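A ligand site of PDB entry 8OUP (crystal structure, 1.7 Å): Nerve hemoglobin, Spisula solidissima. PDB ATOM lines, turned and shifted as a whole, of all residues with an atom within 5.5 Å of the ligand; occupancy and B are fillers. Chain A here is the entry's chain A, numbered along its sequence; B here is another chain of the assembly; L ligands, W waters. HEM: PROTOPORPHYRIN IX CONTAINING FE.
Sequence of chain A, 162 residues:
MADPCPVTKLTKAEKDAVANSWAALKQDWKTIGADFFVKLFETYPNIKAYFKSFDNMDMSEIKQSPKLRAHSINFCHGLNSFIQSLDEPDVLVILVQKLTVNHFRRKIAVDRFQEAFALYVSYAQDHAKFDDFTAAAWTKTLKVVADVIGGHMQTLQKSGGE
NE2 of His 103 binds FE of the ligand (2.0 Å). An iron atom (FE) of the ligand is bound by a ring nitrogen (NE2) of His 71, 2.0 Å away. The side-chain amide nitrogen (ND2) of Asn 102 of chain B is in hydrogen-bond range of an oxygen (O1A) of the ligand. O2A of the ligand lies within salt-bridge range of NH2 of Arg 106.
ND1 of His 103 lies within hydrogen-bond range of O of Leu 99 of chain A (3.0 Å). O of His 103 lies within hydrogen-bond range of N of Ile 108 (3.2 Å). O of Lys 98 of chain B lies within hydrogen-bond range of ND2 of Asn 102 of chain B, 3.3 Å away. The side-chain amino group (NZ) of Lys 98 of chain B sits at hydrogen-bond distance from the side-chain amide oxygen (OD1) of Asn 74, at 3.1 Å.
CG2 of Ile 47 touches CBC of the ligand, 3.6 Å away. Tyr 50 touches the ligand (O to CMD, 3.3 Å). Phe 51 touches the ligand (CZ to CHD, 3.3 Å). Asn 74 touches the ligand. Phe 75 touches the ligand (CD2 to CAB, 3.4 Å). Gly 78 touches the ligand (CA to CMB, 3.9 Å). Leu 99 of chain A touches the ligand. Ile 108 touches the ligand (CD1 to CHD, 3.7 Å). Arg 112 touches the ligand (CB to CBC, 3.7 Å). Phe 113 touches the ligand (CE2 to CHC, 3.5 Å). CE1 of Phe 117 touches CBB of the ligand, 3.6 Å away. Lys 98 of chain B touches the ligand. Hydrophobic or aromatic side chains within 4 Å of the ligand: Ile 47, Tyr 50, Phe 51, His 71, Phe 75, Leu 99 of chain A, His 103, Ile 108, Phe 113 and Phe 117. Within 4 Å of the ligand: Ile 47, Tyr 50, Phe 51, His 71, Asn 74, Phe 75, Gly 78, Leu 99 of chain A, His 103, Arg 106, Ile 108, Arg 112, Phe 113, Phe 117, Lys 98 of chain B and Asn 102 of chain B.
Water W1 lies within hydrogen-bond range of O2A of the ligand (2.7 Å), O of Lys 98 of chain B (2.9 Å) and OD1 of Asn 102 of chain B (3.4 Å). Water W4 bridges O2D of the ligand (2.9 Å) and OG of Ser 53 (3.2 Å). Water W5 bridges the side-chain amide oxygen of Asn 102 of chain B (3.0 Å) and an oxygen (O2A) of the ligand (3.1 Å).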
ATOM      1  N   LEU A  40      20.392  -1.458  11.912  1.00  0.00           N
ATOM      2  CA  LEU A  40      21.355  -2.316  11.223  1.00  0.00           C
ATOM      3  C   LEU A  40      20.641  -3.349  10.350  1.00  0.00           C
ATOM      4  O   LEU A  40      20.984  -3.535   9.184  1.00  0.00           O
ATOM      5  CB  LEU A  40      22.247  -2.973  12.275  1.00  0.00           C
ATOM      6  CG  LEU A  40      23.365  -3.841  11.732  1.00  0.00           C
ATOM      7  CD1 LEU A  40      24.440  -2.993  11.077  1.00  0.00           C
ATOM      8  CD2 LEU A  40      23.903  -4.666  12.871  1.00  0.00           C
ATOM      9  N   ILE A  47      22.584  -8.977   7.154  1.00  0.00           N
ATOM     10  CA  ILE A  47      23.017  -9.080   8.552  1.00  0.00           C
ATOM     11  C   ILE A  47      21.865  -9.628   9.391  1.00  0.00           C
ATOM     12  O   ILE A  47      22.050 -10.497  10.234  1.00  0.00           O
ATOM     13  CB  ILE A  47      23.561  -7.741   9.075  1.00  0.00           C
ATOM     14  CG1 ILE A  47      24.914  -7.441   8.425  1.00  0.00           C
ATOM     15  CG2 ILE A  47      23.653  -7.778  10.602  1.00  0.00           C
ATOM     16  CD1 ILE A  47      25.491  -6.074   8.716  1.00  0.00           C
ATOM     17  N   TYR A  50      21.550 -13.495   9.445  1.00  0.00           N
ATOM     18  CA  TYR A  50      22.378 -14.358  10.290  1.00  0.00           C
ATOM     19  C   TYR A  50      21.634 -14.762  11.565  1.00  0.00           C
ATOM     20  O   TYR A  50      22.021 -15.704  12.223  1.00  0.00           O
ATOM     21  CB  TYR A  50      23.747 -13.737  10.625  1.00  0.00           C
ATOM     22  CG  TYR A  50      24.673 -13.616   9.438  1.00  0.00           C
ATOM     23  CD1 TYR A  50      25.333 -14.725   8.934  1.00  0.00           C
ATOM     24  CD2 TYR A  50      24.845 -12.437   8.758  1.00  0.00           C
ATOM     25  CE1 TYR A  50      26.124 -14.641   7.811  1.00  0.00           C
ATOM     26  CE2 TYR A  50      25.623 -12.318   7.609  1.00  0.00           C
ATOM     27  CZ  TYR A  50      26.245 -13.458   7.102  1.00  0.00           C
ATOM     28  OH  TYR A  50      27.000 -13.371   5.967  1.00  0.00           O
ATOM     29  N   PHE A  51      20.644 -13.980  11.993  1.00  0.00           N
ATOM     30  CA  PHE A  51      19.868 -14.277  13.177  1.00  0.00           C
ATOM     31  C   PHE A  51      18.618 -15.050  12.768  1.00  0.00           C
ATOM     32  O   PHE A  51      17.573 -14.459  12.501  1.00  0.00           O
ATOM     33  CB  PHE A  51      19.516 -12.996  13.931  1.00  0.00           C
ATOM     34  CG  PHE A  51      20.705 -12.247  14.491  1.00  0.00           C
ATOM     35  CD1 PHE A  51      21.439 -11.385  13.706  1.00  0.00           C
ATOM     36  CD2 PHE A  51      21.142 -12.490  15.783  1.00  0.00           C
ATOM     37  CE1 PHE A  51      22.515 -10.681  14.209  1.00  0.00           C
ATOM     38  CE2 PHE A  51      22.246 -11.805  16.281  1.00  0.00           C
ATOM     39  CZ  PHE A  51      22.911 -10.885  15.517  1.00  0.00           C
ATOM     40  N   SER A  53      16.561 -16.936  14.198  1.00  0.00           N
ATOM     41  CA  SER A  53      15.368 -16.865  15.033  1.00  0.00           C
ATOM     42  C   SER A  53      14.516 -15.630  14.746  1.00  0.00           C
ATOM     43  O   SER A  53      13.502 -15.456  15.422  1.00  0.00           O
ATOM     44  CB  SER A  53      15.729 -16.947  16.493  1.00  0.00           C
ATOM     45  OG  SER A  53      16.210 -15.721  16.984  1.00  0.00           O
ATOM     46  N   HIS A  71      22.116 -10.185  22.453  1.00  0.00           N
ATOM     47  CA  HIS A  71      23.183  -9.864  21.516  1.00  0.00           C
ATOM     48  C   HIS A  71      23.623  -8.409  21.702  1.00  0.00           C
ATOM     49  O   HIS A  71      24.795  -8.072  21.540  1.00  0.00           O
ATOM     50  CB  HIS A  71      22.850 -10.163  20.053  1.00  0.00           C
ATOM     51  CG  HIS A  71      24.048 -10.054  19.138  1.00  0.00           C
ATOM     52  ND1 HIS A  71      24.379  -8.904  18.470  1.00  0.00           N
ATOM     53  CD2 HIS A  71      25.070 -10.930  18.919  1.00  0.00           C
ATOM     54  CE1 HIS A  71      25.522  -9.082  17.826  1.00  0.00           C
ATOM     55  NE2 HIS A  71      25.997 -10.340  18.090  1.00  0.00           N
ATOM     56  N   ASN A  74      25.884  -8.318  24.542  1.00  0.00           N
ATOM     57  CA  ASN A  74      27.128  -8.932  24.142  1.00  0.00           C
ATOM     58  C   ASN A  74      27.957  -7.942  23.321  1.00  0.00           C
ATOM     59  O   ASN A  74      29.162  -7.863  23.487  1.00  0.00           O
ATOM     60  CB  ASN A  74      26.918 -10.218  23.376  1.00  0.00           C
ATOM     61  CG  ASN A  74      26.646 -11.413  24.277  1.00  0.00           C
ATOM     62  OD1 ASN A  74      25.937 -12.308  23.820  1.00  0.00           O
ATOM     63  ND2 ASN A  74      27.116 -11.401  25.502  1.00  0.00           N
ATOM     64  N   PHE A  75      27.295  -7.200  22.459  1.00  0.00           N
ATOM     65  CA  PHE A  75      27.946  -6.190  21.637  1.00  0.00           C
ATOM     66  C   PHE A  75      28.579  -5.106  22.497  1.00  0.00           C
ATOM     67  O   PHE A  75      29.759  -4.742  22.344  1.00  0.00           O
ATOM     68  CB  PHE A  75      26.920  -5.666  20.608  1.00  0.00           C
ATOM     69  CG  PHE A  75      27.392  -4.500  19.776  1.00  0.00           C
ATOM     70  CD1 PHE A  75      27.219  -3.198  20.225  1.00  0.00           C
ATOM     71  CD2 PHE A  75      27.989  -4.681  18.535  1.00  0.00           C
ATOM     72  CE1 PHE A  75      27.630  -2.110  19.477  1.00  0.00           C
ATOM     73  CE2 PHE A  75      28.351  -3.580  17.760  1.00  0.00           C
ATOM     74  CZ  PHE A  75      28.247  -2.294  18.262  1.00  0.00           C
ATOM     75  N   GLY A  78      31.504  -6.588  24.520  1.00  0.00           N
ATOM     76  CA  GLY A  78      32.649  -6.824  23.660  1.00  0.00           C
ATOM     77  C   GLY A  78      33.372  -5.529  23.344  1.00  0.00           C
ATOM     78  O   GLY A  78      34.587  -5.385  23.569  1.00  0.00           O
ATOM     79  N   LEU A  79      32.614  -4.498  22.934  1.00  0.00           N
ATOM     80  CA  LEU A  79      33.216  -3.224  22.652  1.00  0.00           C
ATOM     81  C   LEU A  79      33.909  -2.684  23.912  1.00  0.00           C
ATOM     82  O   LEU A  79      35.036  -2.193  23.850  1.00  0.00           O
ATOM     83  CB  LEU A  79      32.081  -2.337  22.121  1.00  0.00           C
ATOM     84  CG  LEU A  79      32.511  -0.983  21.605  1.00  0.00           C
ATOM     85  CD1 LEU A  79      33.595  -1.146  20.558  1.00  0.00           C
ATOM     86  CD2 LEU A  79      31.315  -0.226  21.057  1.00  0.00           C
ATOM     87  N   PHE A  82      37.255  -4.260  24.408  1.00  0.00           N
ATOM     88  CA  PHE A  82      38.250  -3.767  23.452  1.00  0.00           C
ATOM     89  C   PHE A  82      38.779  -2.417  23.894  1.00  0.00           C
ATOM     90  O   PHE A  82      40.008  -2.202  23.934  1.00  0.00           O
ATOM     91  CB  PHE A  82      37.689  -3.739  22.032  1.00  0.00           C
ATOM     92  CG  PHE A  82      37.100  -5.045  21.547  1.00  0.00           C
ATOM     93  CD1 PHE A  82      37.483  -6.275  22.060  1.00  0.00           C
ATOM     94  CD2 PHE A  82      36.140  -5.045  20.544  1.00  0.00           C
ATOM     95  CE1 PHE A  82      36.860  -7.431  21.647  1.00  0.00           C
ATOM     96  CE2 PHE A  82      35.517  -6.201  20.132  1.00  0.00           C
ATOM     97  CZ  PHE A  82      35.901  -7.406  20.666  1.00  0.00           C
ATOM     98  N   LEU A  99      36.313 -13.242  19.382  1.00  0.00           N
ATOM     99  CA  LEU A  99      35.144 -12.785  18.630  1.00  0.00           C
ATOM    100  C   LEU A  99      35.122 -13.306  17.192  1.00  0.00           C
ATOM    101  O   LEU A  99      34.109 -13.708  16.624  1.00  0.00           O
ATOM    102  CB  LEU A  99      35.209 -11.245  18.581  1.00  0.00           C
ATOM    103  CG  LEU A  99      34.037 -10.553  17.887  1.00  0.00           C
ATOM    104  CD1 LEU A  99      32.864 -10.556  18.820  1.00  0.00           C
ATOM    105  CD2 LEU A  99      34.387  -9.152  17.457  1.00  0.00           C
ATOM    106  N   ASN A 102      34.242 -17.172  16.656  1.00  0.00           N
ATOM    107  CA  ASN A 102      32.845 -17.493  16.839  1.00  0.00           C
ATOM    108  C   ASN A 102      32.030 -17.014  15.634  1.00  0.00           C
ATOM    109  O   ASN A 102      31.186 -17.744  15.105  1.00  0.00           O
ATOM    110  CB  ASN A 102      32.334 -16.941  18.172  1.00  0.00           C
ATOM    111  CG  ASN A 102      33.052 -17.493  19.382  1.00  0.00           C
ATOM    112  OD1 ASN A 102      33.419 -18.668  19.408  1.00  0.00           O
ATOM    113  ND2 ASN A 102      33.254 -16.667  20.400  1.00  0.00           N
ATOM    114  N   HIS A 103      32.296 -15.799  15.147  1.00  0.00           N
ATOM    115  CA  HIS A 103      31.468 -15.272  14.068  1.00  0.00           C
ATOM    116  C   HIS A 103      31.880 -15.892  12.731  1.00  0.00           C
ATOM    117  O   HIS A 103      31.044 -16.082  11.849  1.00  0.00           O
ATOM    118  CB  HIS A 103      31.477 -13.724  14.104  1.00  0.00           C
ATOM    119  CG  HIS A 103      30.735 -13.132  15.269  1.00  0.00           C
ATOM    120  ND1 HIS A 103      31.207 -13.070  16.571  1.00  0.00           N
ATOM    121  CD2 HIS A 103      29.484 -12.586  15.305  1.00  0.00           C
ATOM    122  CE1 HIS A 103      30.312 -12.458  17.338  1.00  0.00           C
ATOM    123  NE2 HIS A 103      29.218 -12.188  16.587  1.00  0.00           N
ATOM    124  N   ARG A 106      30.028 -18.893  11.903  1.00  0.00           N
ATOM    125  CA  ARG A 106      28.687 -18.615  11.433  1.00  0.00           C
ATOM    126  C   ARG A 106      28.699 -18.034  10.022  1.00  0.00           C
ATOM    127  O   ARG A 106      27.649 -17.636   9.528  1.00  0.00           O
ATOM    128  CB  ARG A 106      27.974 -17.585  12.297  1.00  0.00           C
ATOM    129  CG  ARG A 106      28.216 -17.729  13.784  1.00  0.00           C
ATOM    130  CD  ARG A 106      27.349 -16.785  14.585  1.00  0.00           C
ATOM    131  NE  ARG A 106      27.224 -17.318  15.922  1.00  0.00           N
ATOM    132  CZ  ARG A 106      28.015 -17.003  16.925  1.00  0.00           C
ATOM    133  NH1 ARG A 106      28.761 -15.895  16.870  1.00  0.00           N
ATOM    134  NH2 ARG A 106      28.089 -17.802  17.973  1.00  0.00           N
ATOM    135  N   ILE A 108      30.177 -15.359   8.871  1.00  0.00           N
ATOM    136  CA  ILE A 108      30.135 -13.903   8.836  1.00  0.00           C
ATOM    137  C   ILE A 108      31.505 -13.388   8.408  1.00  0.00           C
ATOM    138  O   ILE A 108      32.509 -13.767   9.012  1.00  0.00           O
ATOM    139  CB  ILE A 108      29.701 -13.396  10.232  1.00  0.00           C
ATOM    140  CG1 ILE A 108      28.286 -13.837  10.614  1.00  0.00           C
ATOM    141  CG2 ILE A 108      29.834 -11.860  10.354  1.00  0.00           C
ATOM    142  CD1 ILE A 108      27.928 -13.683  12.072  1.00  0.00           C
ATOM    143  N   ARG A 112      30.915  -7.587   7.251  1.00  0.00           N
ATOM    144  CA  ARG A 112      29.683  -7.385   8.029  1.00  0.00           C
ATOM    145  C   ARG A 112      30.015  -6.543   9.267  1.00  0.00           C
ATOM    146  O   ARG A 112      29.266  -5.654   9.655  1.00  0.00           O
ATOM    147  CB  ARG A 112      28.990  -8.662   8.456  1.00  0.00           C
ATOM    148  CG  ARG A 112      28.611  -9.672   7.360  1.00  0.00           C
ATOM    149  CD  ARG A 112      27.722  -9.113   6.243  1.00  0.00           C
ATOM    150  NE  ARG A 112      28.233  -8.158   5.288  1.00  0.00           N
ATOM    151  CZ  ARG A 112      28.877  -8.482   4.164  1.00  0.00           C
ATOM    152  NH1 ARG A 112      29.300  -9.733   3.952  1.00  0.00           N
ATOM    153  NH2 ARG A 112      29.054  -7.578   3.263  1.00  0.00           N
ATOM    154  N   PHE A 113      31.169  -6.828   9.883  1.00  0.00           N
ATOM    155  CA  PHE A 113      31.620  -6.003  11.005  1.00  0.00           C
ATOM    156  C   PHE A 113      31.926  -4.583  10.561  1.00  0.00           C
ATOM    157  O   PHE A 113      31.615  -3.624  11.290  1.00  0.00           O
ATOM    158  CB  PHE A 113      32.849  -6.611  11.698  1.00  0.00           C
ATOM    159  CG  PHE A 113      32.546  -7.837  12.493  1.00  0.00           C
ATOM    160  CD1 PHE A 113      32.651  -9.095  11.913  1.00  0.00           C
ATOM    161  CD2 PHE A 113      32.262  -7.732  13.843  1.00  0.00           C
ATOM    162  CE1 PHE A 113      32.354 -10.221  12.671  1.00  0.00           C
ATOM    163  CE2 PHE A 113      31.974  -8.860  14.598  1.00  0.00           C
ATOM    164  CZ  PHE A 113      32.079 -10.118  14.019  1.00  0.00           C
ATOM    165  N   ALA A 116      28.609  -2.880  10.336  1.00  0.00           N
ATOM    166  CA  ALA A 116      28.086  -2.577  11.667  1.00  0.00           C
ATOM    167  C   ALA A 116      28.836  -1.440  12.340  1.00  0.00           C
ATOM    168  O   ALA A 116      28.228  -0.591  12.943  1.00  0.00           O
ATOM    169  CB  ALA A 116      28.103  -3.796  12.549  1.00  0.00           C
ATOM    170  N   PHE A 117      30.167  -1.456  12.231  1.00  0.00           N
ATOM    171  CA  PHE A 117      31.001  -0.454  12.903  1.00  0.00           C
ATOM    172  C   PHE A 117      30.717   0.939  12.345  1.00  0.00           C
ATOM    173  O   PHE A 117      30.539   1.912  13.078  1.00  0.00           O
ATOM    174  CB  PHE A 117      32.477  -0.814  12.742  1.00  0.00           C
ATOM    175  CG  PHE A 117      32.933  -2.002  13.545  1.00  0.00           C
ATOM    176  CD1 PHE A 117      32.151  -2.557  14.530  1.00  0.00           C
ATOM    177  CD2 PHE A 117      34.196  -2.553  13.325  1.00  0.00           C
ATOM    178  CE1 PHE A 117      32.584  -3.641  15.272  1.00  0.00           C
ATOM    179  CE2 PHE A 117      34.624  -3.642  14.055  1.00  0.00           C
ATOM    180  CZ  PHE A 117      33.832  -4.169  15.031  1.00  0.00           C
ATOM    181  N   LYS B  98      24.853 -19.189  26.766  1.00  0.00           N
ATOM    182  CA  LYS B  98      25.891 -19.022  25.760  1.00  0.00           C
ATOM    183  C   LYS B  98      27.269 -19.280  26.363  1.00  0.00           C
ATOM    184  O   LYS B  98      28.107 -19.989  25.794  1.00  0.00           O
ATOM    185  CB  LYS B  98      25.822 -17.613  25.163  1.00  0.00           C
ATOM    186  CG  LYS B  98      24.673 -17.293  24.224  1.00  0.00           C
ATOM    187  CD  LYS B  98      24.741 -15.852  23.763  1.00  0.00           C
ATOM    188  CE  LYS B  98      23.626 -15.372  22.872  1.00  0.00           C
ATOM    189  NZ  LYS B  98      23.888 -14.003  22.295  1.00  0.00           N
ATOM    190  N   LEU B  99      27.513 -18.753  27.567  1.00  0.00           N
ATOM    191  CA  LEU B  99      28.726 -19.067  28.312  1.00  0.00           C
ATOM    192  C   LEU B  99      28.882 -20.560  28.480  1.00  0.00           C
ATOM    193  O   LEU B  99      29.965 -21.130  28.343  1.00  0.00           O
ATOM    194  CB  LEU B  99      28.616 -18.410  29.698  1.00  0.00           C
ATOM    195  CG  LEU B  99      29.668 -18.843  30.726  1.00  0.00           C
ATOM    196  CD1 LEU B  99      30.878 -18.002  30.569  1.00  0.00           C
ATOM    197  CD2 LEU B  99      29.144 -18.796  32.159  1.00  0.00           C
ATOM    198  N   ASN B 102      29.975 -22.680  25.357  1.00  0.00           N
ATOM    199  CA  ASN B 102      31.387 -22.503  25.008  1.00  0.00           C
ATOM    200  C   ASN B 102      32.296 -23.308  25.935  1.00  0.00           C
ATOM    201  O   ASN B 102      33.255 -23.959  25.505  1.00  0.00           O
ATOM    202  CB  ASN B 102      31.791 -21.043  24.992  1.00  0.00           C
ATOM    203  CG  ASN B 102      31.134 -20.267  23.875  1.00  0.00           C
ATOM    204  OD1 ASN B 102      30.953 -20.788  22.757  1.00  0.00           O
ATOM    205  ND2 ASN B 102      30.849 -19.010  24.142  1.00  0.00           N
HETATM  206  CHA HEM L   1      26.588 -14.012  18.887  1.00  0.00           C
HETATM  207  CHB HEM L   1      29.420 -10.325  20.100  1.00  0.00           C
HETATM  208  CHC HEM L   1      28.671  -8.440  15.722  1.00  0.00           C
HETATM  209  CHD HEM L   1      25.789 -12.086  14.562  1.00  0.00           C
HETATM  210  C1A HEM L   1      27.443 -13.219  19.541  1.00  0.00           C
HETATM  211  C2A HEM L   1      27.998 -13.506  20.795  1.00  0.00           C
HETATM  212  C3A HEM L   1      28.794 -12.454  21.140  1.00  0.00           C
HETATM  213  C4A HEM L   1      28.723 -11.525  20.125  1.00  0.00           C
HETATM  214  CMA HEM L   1      29.615 -12.324  22.391  1.00  0.00           C
HETATM  215  CAA HEM L   1      27.791 -14.777  21.579  1.00  0.00           C
HETATM  216  CBA HEM L   1      28.985 -15.661  21.144  1.00  0.00           C
HETATM  217  CGA HEM L   1      29.035 -16.985  21.860  1.00  0.00           C
HETATM  218  O1A HEM L   1      29.380 -17.040  23.068  1.00  0.00           O
HETATM  219  O2A HEM L   1      28.731 -18.012  21.218  1.00  0.00           O
HETATM  220  C1B HEM L   1      29.432  -9.449  19.041  1.00  0.00           C
HETATM  221  C2B HEM L   1      30.217  -8.230  19.012  1.00  0.00           C
HETATM  222  C3B HEM L   1      30.022  -7.691  17.772  1.00  0.00           C
HETATM  223  C4B HEM L   1      29.090  -8.600  17.043  1.00  0.00           C
HETATM  224  CMB HEM L   1      31.060  -7.771  20.187  1.00  0.00           C
HETATM  225  CAB HEM L   1      30.587  -6.449  17.207  1.00  0.00           C
HETATM  226  CBB HEM L   1      31.406  -5.733  18.017  1.00  0.00           C
HETATM  227  C1C HEM L   1      27.852  -9.250  14.961  1.00  0.00           C
HETATM  228  C2C HEM L   1      27.518  -9.091  13.605  1.00  0.00           C
HETATM  229  C3C HEM L   1      26.635 -10.109  13.332  1.00  0.00           C
HETATM  230  C4C HEM L   1      26.536 -10.926  14.484  1.00  0.00           C
HETATM  231  CMC HEM L   1      27.997  -7.923  12.728  1.00  0.00           C
HETATM  232  CAC HEM L   1      26.031 -10.510  12.041  1.00  0.00           C
HETATM  233  CBC HEM L   1      26.510  -9.935  10.909  1.00  0.00           C
HETATM  234  C1D HEM L   1      25.773 -12.914  15.676  1.00  0.00           C
HETATM  235  C2D HEM L   1      24.958 -14.112  15.733  1.00  0.00           C
HETATM  236  C3D HEM L   1      25.182 -14.658  16.906  1.00  0.00           C
HETATM  237  C4D HEM L   1      26.142 -13.766  17.598  1.00  0.00           C
HETATM  238  CMD HEM L   1      24.085 -14.563  14.592  1.00  0.00           C
HETATM  239  CAD HEM L   1      24.490 -15.896  17.440  1.00  0.00           C
HETATM  240  CBD HEM L   1      23.217 -15.331  18.127  1.00  0.00           C
HETATM  241  CGD HEM L   1      22.216 -16.390  18.572  1.00  0.00           C
HETATM  242  O1D HEM L   1      22.248 -16.813  19.714  1.00  0.00           O
HETATM  243  O2D HEM L   1      21.352 -16.844  17.808  1.00  0.00           O
HETATM  244  NA  HEM L   1      27.884 -11.991  19.092  1.00  0.00           N
HETATM  245  NB  HEM L   1      28.799  -9.616  17.892  1.00  0.00           N
HETATM  246  NC  HEM L   1      27.313 -10.385  15.420  1.00  0.00           N
HETATM  247  ND  HEM L   1      26.480 -12.693  16.829  1.00  0.00           N
HETATM  248 FE   HEM L   1      27.626 -11.227  17.327  1.00  0.00          FE
HETATM  249  O   HOH W   1      27.723 -19.795  22.910  1.00  0.00           O
HETATM  250  O   HOH W   2      19.813 -16.106  21.573  1.00  0.00           O
HETATM  251  O   HOH W   3      28.623 -14.935  25.201  1.00  0.00           O
HETATM  252  O   HOH W   4      19.191 -16.077  15.983  1.00  0.00           O
HETATM  253  O   HOH W   5      28.959 -21.020  20.594  1.00  0.00           O
